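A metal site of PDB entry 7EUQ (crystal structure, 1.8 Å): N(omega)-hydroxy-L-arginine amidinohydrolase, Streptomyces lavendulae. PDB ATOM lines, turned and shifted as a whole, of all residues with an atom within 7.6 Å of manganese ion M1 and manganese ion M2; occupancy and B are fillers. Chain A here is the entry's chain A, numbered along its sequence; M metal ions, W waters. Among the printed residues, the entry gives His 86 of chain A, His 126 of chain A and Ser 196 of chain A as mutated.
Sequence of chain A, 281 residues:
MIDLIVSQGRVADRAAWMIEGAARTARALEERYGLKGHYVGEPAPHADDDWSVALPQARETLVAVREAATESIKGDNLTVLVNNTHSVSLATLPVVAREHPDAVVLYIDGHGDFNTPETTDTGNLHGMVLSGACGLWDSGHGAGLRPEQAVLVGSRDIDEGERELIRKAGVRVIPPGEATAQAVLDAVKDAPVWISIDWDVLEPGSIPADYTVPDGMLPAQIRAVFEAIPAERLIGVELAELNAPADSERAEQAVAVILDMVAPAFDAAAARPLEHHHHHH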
ATOM      1  N   THR A  85       1.527 -29.128 -24.425  1.00  0.00           N
ATOM      2  CA  THR A  85       1.100 -28.411 -23.198  1.00  0.00           C
ATOM      3  C   THR A  85       2.140 -28.552 -22.092  1.00  0.00           C
ATOM      4  O   THR A  85       2.858 -29.583 -22.035  1.00  0.00           O
ATOM      5  CB  THR A  85      -0.263 -28.911 -22.721  1.00  0.00           C
ATOM      6  OG1 THR A  85      -0.717 -28.000 -21.709  1.00  0.00           O
ATOM      7  CG2 THR A  85      -0.193 -30.305 -22.166  1.00  0.00           C
ATOM      8  N   HIS A  86       2.133 -27.625 -21.145  1.00  0.00           N
ATOM      9  CA  HIS A  86       3.004 -27.691 -19.944  1.00  0.00           C
ATOM     10  C   HIS A  86       2.646 -28.925 -19.127  1.00  0.00           C
ATOM     11  O   HIS A  86       3.507 -29.435 -18.429  1.00  0.00           O
ATOM     12  CB  HIS A  86       2.929 -26.432 -19.070  1.00  0.00           C
ATOM     13  CG  HIS A  86       4.259 -26.107 -18.468  1.00  0.00           C
ATOM     14  ND1 HIS A  86       4.506 -24.919 -17.824  1.00  0.00           N
ATOM     15  CD2 HIS A  86       5.430 -26.788 -18.477  1.00  0.00           C
ATOM     16  CE1 HIS A  86       5.756 -24.918 -17.426  1.00  0.00           C
ATOM     17  NE2 HIS A  86       6.352 -26.036 -17.813  1.00  0.00           N
ATOM     18  N   SER A  87       1.419 -29.421 -19.224  1.00  0.00           N
ATOM     19  CA  SER A  87       0.903 -30.526 -18.398  1.00  0.00           C
ATOM     20  C   SER A  87       1.701 -31.817 -18.639  1.00  0.00           C
ATOM     21  O   SER A  87       1.673 -32.688 -17.770  1.00  0.00           O
ATOM     22  CB  SER A  87      -0.575 -30.711 -18.631  1.00  0.00           C
ATOM     23  OG  SER A  87      -1.291 -29.681 -18.001  1.00  0.00           O
ATOM     24  N   TYR A 107      11.946 -23.720 -13.825  1.00  0.00           N
ATOM     25  CA  TYR A 107      10.553 -23.758 -14.311  1.00  0.00           C
ATOM     26  C   TYR A 107      10.217 -22.354 -14.775  1.00  0.00           C
ATOM     27  O   TYR A 107       9.875 -21.469 -13.939  1.00  0.00           O
ATOM     28  CB  TYR A 107       9.633 -24.331 -13.239  1.00  0.00           C
ATOM     29  CG  TYR A 107       8.271 -24.775 -13.697  1.00  0.00           C
ATOM     30  CD1 TYR A 107       7.209 -23.885 -13.785  1.00  0.00           C
ATOM     31  CD2 TYR A 107       8.017 -26.110 -13.939  1.00  0.00           C
ATOM     32  CE1 TYR A 107       5.942 -24.318 -14.153  1.00  0.00           C
ATOM     33  CE2 TYR A 107       6.751 -26.558 -14.291  1.00  0.00           C
ATOM     34  CZ  TYR A 107       5.726 -25.655 -14.439  1.00  0.00           C
ATOM     35  OH  TYR A 107       4.495 -26.156 -14.771  1.00  0.00           O
ATOM     36  N   ILE A 108      10.405 -22.143 -16.078  1.00  0.00           N
ATOM     37  CA  ILE A 108      10.396 -20.799 -16.690  1.00  0.00           C
ATOM     38  C   ILE A 108       8.964 -20.561 -17.177  1.00  0.00           C
ATOM     39  O   ILE A 108       8.562 -21.156 -18.198  1.00  0.00           O
ATOM     40  CB  ILE A 108      11.453 -20.642 -17.786  1.00  0.00           C
ATOM     41  CG1 ILE A 108      12.857 -21.061 -17.314  1.00  0.00           C
ATOM     42  CG2 ILE A 108      11.424 -19.222 -18.309  1.00  0.00           C
ATOM     43  CD1 ILE A 108      13.940 -20.772 -18.323  1.00  0.00           C
ATOM     44  N   ASP A 109       8.259 -19.659 -16.518  1.00  0.00           N
ATOM     45  CA  ASP A 109       6.787 -19.556 -16.649  1.00  0.00           C
ATOM     46  C   ASP A 109       6.304 -18.200 -16.122  1.00  0.00           C
ATOM     47  O   ASP A 109       6.884 -17.726 -15.123  1.00  0.00           O
ATOM     48  CB  ASP A 109       6.193 -20.701 -15.826  1.00  0.00           C
ATOM     49  CG  ASP A 109       4.800 -21.101 -16.246  1.00  0.00           C
ATOM     50  OD1 ASP A 109       3.952 -20.201 -16.442  1.00  0.00           O
ATOM     51  OD2 ASP A 109       4.602 -22.321 -16.428  1.00  0.00           O
ATOM     52  N   GLY A 110       5.239 -17.699 -16.712  1.00  0.00           N
ATOM     53  CA  GLY A 110       4.538 -16.475 -16.277  1.00  0.00           C
ATOM     54  C   GLY A 110       3.738 -16.709 -14.998  1.00  0.00           C
ATOM     55  O   GLY A 110       3.345 -15.707 -14.378  1.00  0.00           O
ATOM     56  N   HIS A 111       3.485 -17.973 -14.644  1.00  0.00           N
ATOM     57  CA  HIS A 111       2.619 -18.400 -13.514  1.00  0.00           C
ATOM     58  C   HIS A 111       3.402 -19.321 -12.577  1.00  0.00           C
ATOM     59  O   HIS A 111       4.551 -19.663 -12.901  1.00  0.00           O
ATOM     60  CB  HIS A 111       1.360 -19.113 -14.052  1.00  0.00           C
ATOM     61  CG  HIS A 111       0.613 -18.361 -15.096  1.00  0.00           C
ATOM     62  ND1 HIS A 111       0.845 -18.556 -16.456  1.00  0.00           N
ATOM     63  CD2 HIS A 111      -0.378 -17.456 -14.998  1.00  0.00           C
ATOM     64  CE1 HIS A 111       0.046 -17.764 -17.137  1.00  0.00           C
ATOM     65  NE2 HIS A 111      -0.702 -17.061 -16.259  1.00  0.00           N
ATOM     66  N   GLY A 112       2.815 -19.717 -11.435  1.00  0.00           N
ATOM     67  CA  GLY A 112       3.468 -20.678 -10.544  1.00  0.00           C
ATOM     68  C   GLY A 112       3.148 -22.135 -10.865  1.00  0.00           C
ATOM     69  O   GLY A 112       3.926 -22.987 -10.417  1.00  0.00           O
ATOM     70  N   ASP A 113       2.014 -22.409 -11.493  1.00  0.00           N
ATOM     71  CA  ASP A 113       1.530 -23.778 -11.768  1.00  0.00           C
ATOM     72  C   ASP A 113       1.593 -24.584 -10.477  1.00  0.00           C
ATOM     73  O   ASP A 113       1.973 -25.761 -10.522  1.00  0.00           O
ATOM     74  CB  ASP A 113       2.278 -24.427 -12.925  1.00  0.00           C
ATOM     75  CG  ASP A 113       2.089 -23.721 -14.248  1.00  0.00           C
ATOM     76  OD1 ASP A 113       1.287 -22.785 -14.309  1.00  0.00           O
ATOM     77  OD2 ASP A 113       2.704 -24.174 -15.230  1.00  0.00           O
ATOM     78  N   HIS A 126      -3.199 -27.467 -15.978  1.00  0.00           N
ATOM     79  CA  HIS A 126      -1.963 -26.702 -16.244  1.00  0.00           C
ATOM     80  C   HIS A 126      -1.545 -25.963 -14.968  1.00  0.00           C
ATOM     81  O   HIS A 126      -0.376 -26.008 -14.613  1.00  0.00           O
ATOM     82  CB  HIS A 126      -2.151 -25.759 -17.456  1.00  0.00           C
ATOM     83  CG  HIS A 126      -0.910 -25.035 -17.857  1.00  0.00           C
ATOM     84  ND1 HIS A 126      -0.874 -24.179 -18.934  1.00  0.00           N
ATOM     85  CD2 HIS A 126       0.337 -25.037 -17.328  1.00  0.00           C
ATOM     86  CE1 HIS A 126       0.320 -23.690 -19.069  1.00  0.00           C
ATOM     87  NE2 HIS A 126       1.086 -24.181 -18.075  1.00  0.00           N
ATOM     88  N   GLY A 127      -2.487 -25.361 -14.248  1.00  0.00           N
ATOM     89  CA  GLY A 127      -2.174 -24.610 -13.027  1.00  0.00           C
ATOM     90  C   GLY A 127      -1.694 -25.479 -11.886  1.00  0.00           C
ATOM     91  O   GLY A 127      -1.544 -24.935 -10.772  1.00  0.00           O
ATOM     92  N   VAL A 129       0.673 -28.281 -12.318  1.00  0.00           N
ATOM     93  CA  VAL A 129       1.757 -29.158 -12.838  1.00  0.00           C
ATOM     94  C   VAL A 129       2.914 -29.208 -11.857  1.00  0.00           C
ATOM     95  O   VAL A 129       3.334 -30.343 -11.524  1.00  0.00           O
ATOM     96  CB  VAL A 129       2.224 -28.709 -14.233  1.00  0.00           C
ATOM     97  CG1 VAL A 129       3.497 -29.452 -14.618  1.00  0.00           C
ATOM     98  CG2 VAL A 129       1.130 -28.869 -15.241  1.00  0.00           C
ATOM     99  N   LEU A 130       3.445 -28.069 -11.408  1.00  0.00           N
ATOM    100  CA  LEU A 130       4.678 -28.055 -10.584  1.00  0.00           C
ATOM    101  C   LEU A 130       4.368 -28.597  -9.190  1.00  0.00           C
ATOM    102  O   LEU A 130       5.175 -29.359  -8.682  1.00  0.00           O
ATOM    103  CB  LEU A 130       5.278 -26.646 -10.511  1.00  0.00           C
ATOM    104  CG  LEU A 130       6.619 -26.518  -9.779  1.00  0.00           C
ATOM    105  CD1 LEU A 130       7.643 -27.531 -10.276  1.00  0.00           C
ATOM    106  CD2 LEU A 130       7.145 -25.086  -9.906  1.00  0.00           C
ATOM    107  N   ARG A 156       4.871 -13.901 -12.643  1.00  0.00           N
ATOM    108  CA  ARG A 156       4.350 -12.571 -12.255  1.00  0.00           C
ATOM    109  C   ARG A 156       2.857 -12.608 -11.912  1.00  0.00           C
ATOM    110  O   ARG A 156       2.364 -11.582 -11.427  1.00  0.00           O
ATOM    111  CB  ARG A 156       4.535 -11.588 -13.399  1.00  0.00           C
ATOM    112  CG  ARG A 156       3.898 -12.074 -14.691  1.00  0.00           C
ATOM    113  CD  ARG A 156       4.597 -11.425 -15.850  1.00  0.00           C
ATOM    114  NE  ARG A 156       4.196 -11.979 -17.124  1.00  0.00           N
ATOM    115  CZ  ARG A 156       4.916 -12.851 -17.849  1.00  0.00           C
ATOM    116  NH1 ARG A 156       6.116 -13.287 -17.428  1.00  0.00           N
ATOM    117  NH2 ARG A 156       4.428 -13.213 -19.023  1.00  0.00           N
ATOM    118  N   ASP A 157       2.198 -13.730 -12.148  1.00  0.00           N
ATOM    119  CA  ASP A 157       0.736 -13.898 -11.927  1.00  0.00           C
ATOM    120  C   ASP A 157       0.555 -15.121 -11.012  1.00  0.00           C
ATOM    121  O   ASP A 157       0.359 -16.227 -11.539  1.00  0.00           O
ATOM    122  CB  ASP A 157       0.029 -13.995 -13.283  1.00  0.00           C
ATOM    123  CG  ASP A 157      -1.490 -13.921 -13.230  1.00  0.00           C
ATOM    124  OD1 ASP A 157      -2.033 -13.795 -12.111  1.00  0.00           O
ATOM    125  OD2 ASP A 157      -2.102 -13.998 -14.307  1.00  0.00           O
ATOM    126  N   SER A 196      12.488 -26.189 -17.979  1.00  0.00           N
ATOM    127  CA  SER A 196      11.089 -26.401 -18.441  1.00  0.00           C
ATOM    128  C   SER A 196      10.463 -25.070 -18.802  1.00  0.00           C
ATOM    129  O   SER A 196      10.253 -24.283 -17.889  1.00  0.00           O
ATOM    130  CB  SER A 196      10.289 -27.159 -17.429  1.00  0.00           C
ATOM    131  OG  SER A 196       8.984 -27.431 -17.902  1.00  0.00           O
ATOM    132  N   ILE A 197      10.237 -24.802 -20.081  1.00  0.00           N
ATOM    133  CA  ILE A 197       9.726 -23.474 -20.531  1.00  0.00           C
ATOM    134  C   ILE A 197       8.242 -23.558 -20.921  1.00  0.00           C
ATOM    135  O   ILE A 197       7.835 -24.451 -21.707  1.00  0.00           O
ATOM    136  CB  ILE A 197      10.580 -22.880 -21.673  1.00  0.00           C
ATOM    137  CG1 ILE A 197      12.014 -22.610 -21.235  1.00  0.00           C
ATOM    138  CG2 ILE A 197       9.929 -21.609 -22.181  1.00  0.00           C
ATOM    139  CD1 ILE A 197      12.943 -22.219 -22.365  1.00  0.00           C
ATOM    140  N   ASP A 198       7.481 -22.580 -20.440  1.00  0.00           N
ATOM    141  CA  ASP A 198       6.122 -22.222 -20.912  1.00  0.00           C
ATOM    142  C   ASP A 198       6.277 -20.864 -21.610  1.00  0.00           C
ATOM    143  O   ASP A 198       6.654 -19.909 -20.933  1.00  0.00           O
ATOM    144  CB  ASP A 198       5.161 -22.233 -19.715  1.00  0.00           C
ATOM    145  CG  ASP A 198       3.744 -21.719 -19.966  1.00  0.00           C
ATOM    146  OD1 ASP A 198       3.493 -21.222 -21.066  1.00  0.00           O
ATOM    147  OD2 ASP A 198       2.933 -21.809 -19.033  1.00  0.00           O
ATOM    148  N   TRP A 199       6.062 -20.790 -22.921  1.00  0.00           N
ATOM    149  CA  TRP A 199       6.240 -19.536 -23.698  1.00  0.00           C
ATOM    150  C   TRP A 199       5.319 -18.413 -23.194  1.00  0.00           C
ATOM    151  O   TRP A 199       5.613 -17.300 -23.532  1.00  0.00           O
ATOM    152  CB  TRP A 199       6.003 -19.743 -25.199  1.00  0.00           C
ATOM    153  CG  TRP A 199       6.930 -20.736 -25.787  1.00  0.00           C
ATOM    154  CD1 TRP A 199       6.618 -21.886 -26.454  1.00  0.00           C
ATOM    155  CD2 TRP A 199       8.365 -20.684 -25.747  1.00  0.00           C
ATOM    156  NE1 TRP A 199       7.757 -22.558 -26.820  1.00  0.00           N
ATOM    157  CE2 TRP A 199       8.845 -21.828 -26.422  1.00  0.00           C
ATOM    158  CE3 TRP A 199       9.278 -19.780 -25.218  1.00  0.00           C
ATOM    159  CZ2 TRP A 199      10.204 -22.110 -26.529  1.00  0.00           C
ATOM    160  CZ3 TRP A 199      10.622 -20.027 -25.370  1.00  0.00           C
ATOM    161  CH2 TRP A 199      11.074 -21.185 -26.017  1.00  0.00           C
ATOM    162  N   ASP A 200       4.302 -18.659 -22.365  1.00  0.00           N
ATOM    163  CA  ASP A 200       3.526 -17.534 -21.781  1.00  0.00           C
ATOM    164  C   ASP A 200       4.419 -16.697 -20.838  1.00  0.00           C
ATOM    165  O   ASP A 200       3.947 -15.606 -20.412  1.00  0.00           O
ATOM    166  CB  ASP A 200       2.185 -17.958 -21.194  1.00  0.00           C
ATOM    167  CG  ASP A 200       2.234 -18.641 -19.832  1.00  0.00           C
ATOM    168  OD1 ASP A 200       3.262 -18.483 -19.090  1.00  0.00           O
ATOM    169  OD2 ASP A 200       1.270 -19.421 -19.559  1.00  0.00           O
ATOM    170  N   VAL A 201       5.659 -17.109 -20.557  1.00  0.00           N
ATOM    171  CA  VAL A 201       6.597 -16.303 -19.733  1.00  0.00           C
ATOM    172  C   VAL A 201       6.966 -15.017 -20.474  1.00  0.00           C
ATOM    173  O   VAL A 201       7.286 -14.008 -19.838  1.00  0.00           O
ATOM    174  CB  VAL A 201       7.869 -17.085 -19.361  1.00  0.00           C
ATOM    175  CG1 VAL A 201       8.786 -17.302 -20.553  1.00  0.00           C
ATOM    176  CG2 VAL A 201       8.594 -16.413 -18.220  1.00  0.00           C
ATOM    177  N   ALA A 209       0.745 -18.189 -26.847  1.00  0.00           N
ATOM    178  CA  ALA A 209       0.416 -19.337 -25.957  1.00  0.00           C
ATOM    179  C   ALA A 209      -1.105 -19.336 -25.702  1.00  0.00           C
ATOM    180  O   ALA A 209      -1.876 -18.814 -26.558  1.00  0.00           O
ATOM    181  CB  ALA A 209       1.229 -19.243 -24.688  1.00  0.00           C
ATOM    182  N   TYR A 211      -2.292 -18.334 -22.424  1.00  0.00           N
ATOM    183  CA  TYR A 211      -2.421 -17.226 -21.456  1.00  0.00           C
ATOM    184  C   TYR A 211      -1.589 -16.021 -21.934  1.00  0.00           C
ATOM    185  O   TYR A 211      -0.497 -16.199 -22.514  1.00  0.00           O
ATOM    186  CB  TYR A 211      -2.051 -17.713 -20.053  1.00  0.00           C
ATOM    187  CG  TYR A 211      -3.109 -18.605 -19.464  1.00  0.00           C
ATOM    188  CD1 TYR A 211      -3.098 -19.974 -19.691  1.00  0.00           C
ATOM    189  CD2 TYR A 211      -4.167 -18.073 -18.756  1.00  0.00           C
ATOM    190  CE1 TYR A 211      -4.096 -20.799 -19.195  1.00  0.00           C
ATOM    191  CE2 TYR A 211      -5.175 -18.882 -18.244  1.00  0.00           C
ATOM    192  CZ  TYR A 211      -5.144 -20.246 -18.463  1.00  0.00           C
ATOM    193  OH  TYR A 211      -6.133 -21.045 -17.956  1.00  0.00           O
ATOM    194  N   VAL A 213      -0.255 -12.469 -20.233  1.00  0.00           N
ATOM    195  CA  VAL A 213      -0.027 -11.739 -18.936  1.00  0.00           C
ATOM    196  C   VAL A 213       1.096 -10.722 -19.136  1.00  0.00           C
ATOM    197  O   VAL A 213       2.212 -11.079 -19.516  1.00  0.00           O
ATOM    198  CB  VAL A 213       0.222 -12.728 -17.772  1.00  0.00           C
ATOM    199  CG1 VAL A 213       1.220 -13.827 -18.149  1.00  0.00           C
ATOM    200  CG2 VAL A 213       0.633 -12.027 -16.481  1.00  0.00           C
ATOM    201  N   ALA A 240       7.187 -25.784 -24.151  1.00  0.00           N
ATOM    202  CA  ALA A 240       5.730 -26.033 -24.112  1.00  0.00           C
ATOM    203  C   ALA A 240       4.971 -24.756 -24.415  1.00  0.00           C
ATOM    204  O   ALA A 240       5.496 -23.699 -24.148  1.00  0.00           O
ATOM    205  CB  ALA A 240       5.359 -26.594 -22.752  1.00  0.00           C
ATOM    206  N   GLU A 241       3.737 -24.927 -24.920  1.00  0.00           N
ATOM    207  CA  GLU A 241       2.680 -23.897 -24.955  1.00  0.00           C
ATOM    208  C   GLU A 241       2.924 -22.922 -26.108  1.00  0.00           C
ATOM    209  O   GLU A 241       2.623 -21.751 -25.933  1.00  0.00           O
ATOM    210  CB  GLU A 241       2.562 -23.189 -23.606  1.00  0.00           C
ATOM    211  CG  GLU A 241       2.256 -24.162 -22.462  1.00  0.00           C
ATOM    212  CD  GLU A 241       0.771 -24.414 -22.228  1.00  0.00           C
ATOM    213  OE1 GLU A 241      -0.027 -23.443 -22.367  1.00  0.00           O
ATOM    214  OE2 GLU A 241       0.421 -25.567 -21.872  1.00  0.00           O
HETATM  215 MN    MN M   1       2.936 -23.385 -17.299  1.00  0.00          MN
HETATM  216 MN    MN M   2       2.131 -20.181 -17.646  1.00  0.00          MN
HETATM  217  O   HOH W   1       1.431 -21.715 -16.689  1.00  0.00           O
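Manganese ion M1 is bound by NE2 of His 126 (2.2 Å), OD2 of Asp 109 (2.2 Å), OD2 of Asp 113 (2.2 Å), ND1 of His 86 (2.3 Å), water W1 (2.3 Å) and OD2 of Asp 198 (2.3 Å). Manganese ion M1 has six donor atoms within binding distance.
Of the 27 residues printed, 4 come within 4 Å of manganese ion M2. Along chain A the residues within 4 Å of manganese ion M2 span positions 109 to 200. The nearest printed residue that does not touch manganese ion M2 is Gly 110 (4.1 Å).
Manganese ion M2 is bound by water W1. OD1 of Asp 109 is bound to manganese ion M2, at 2.2 Å. OD2 of Asp 200 binds manganese ion M2, 2.2 Å away. Manganese ion M2 is bound by OD2 of Asp 198, at 2.3 Å. Manganese ion M2 is bound by a ring nitrogen (ND1) of His 111, 2.4 Å away. The side-chain carboxylate (OD1) of Asp 200 binds manganese ion M2, 2.5 Å away.
A ring nitrogen (ND1) of His 126 lies close to the side-chain carboxylate (OE2) of Glu 241 (3.5 Å). The side-chain hydroxyl (OH) of Tyr 107 sits close to the side-chain carboxylate (OD2) of Asp 113, at 2.7 Å. N of Val 129 is in hydrogen-bond range of O of Asp 113. The backbone carbonyl oxygen (O) of Asp 113 lies within hydrogen-bond range of the backbone NH (N) of Leu 130, 2.9 Å away. OD1 of Asp 200 sits close to N of Gly 110. The guanidinium group of Arg 156 sits at hydrogen-bond distance from the backbone carbonyl oxygen of Asp 200 (2.8 Å). The backbone NH of His 86 lies within hydrogen-bond range of the side-chain carboxylate of Glu 241 (2.8 Å). The backbone NH (N) of Asp 198 sits at hydrogen-bond distance from the backbone carbonyl oxygen (O) of Ile 108, 2.9 Å away.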
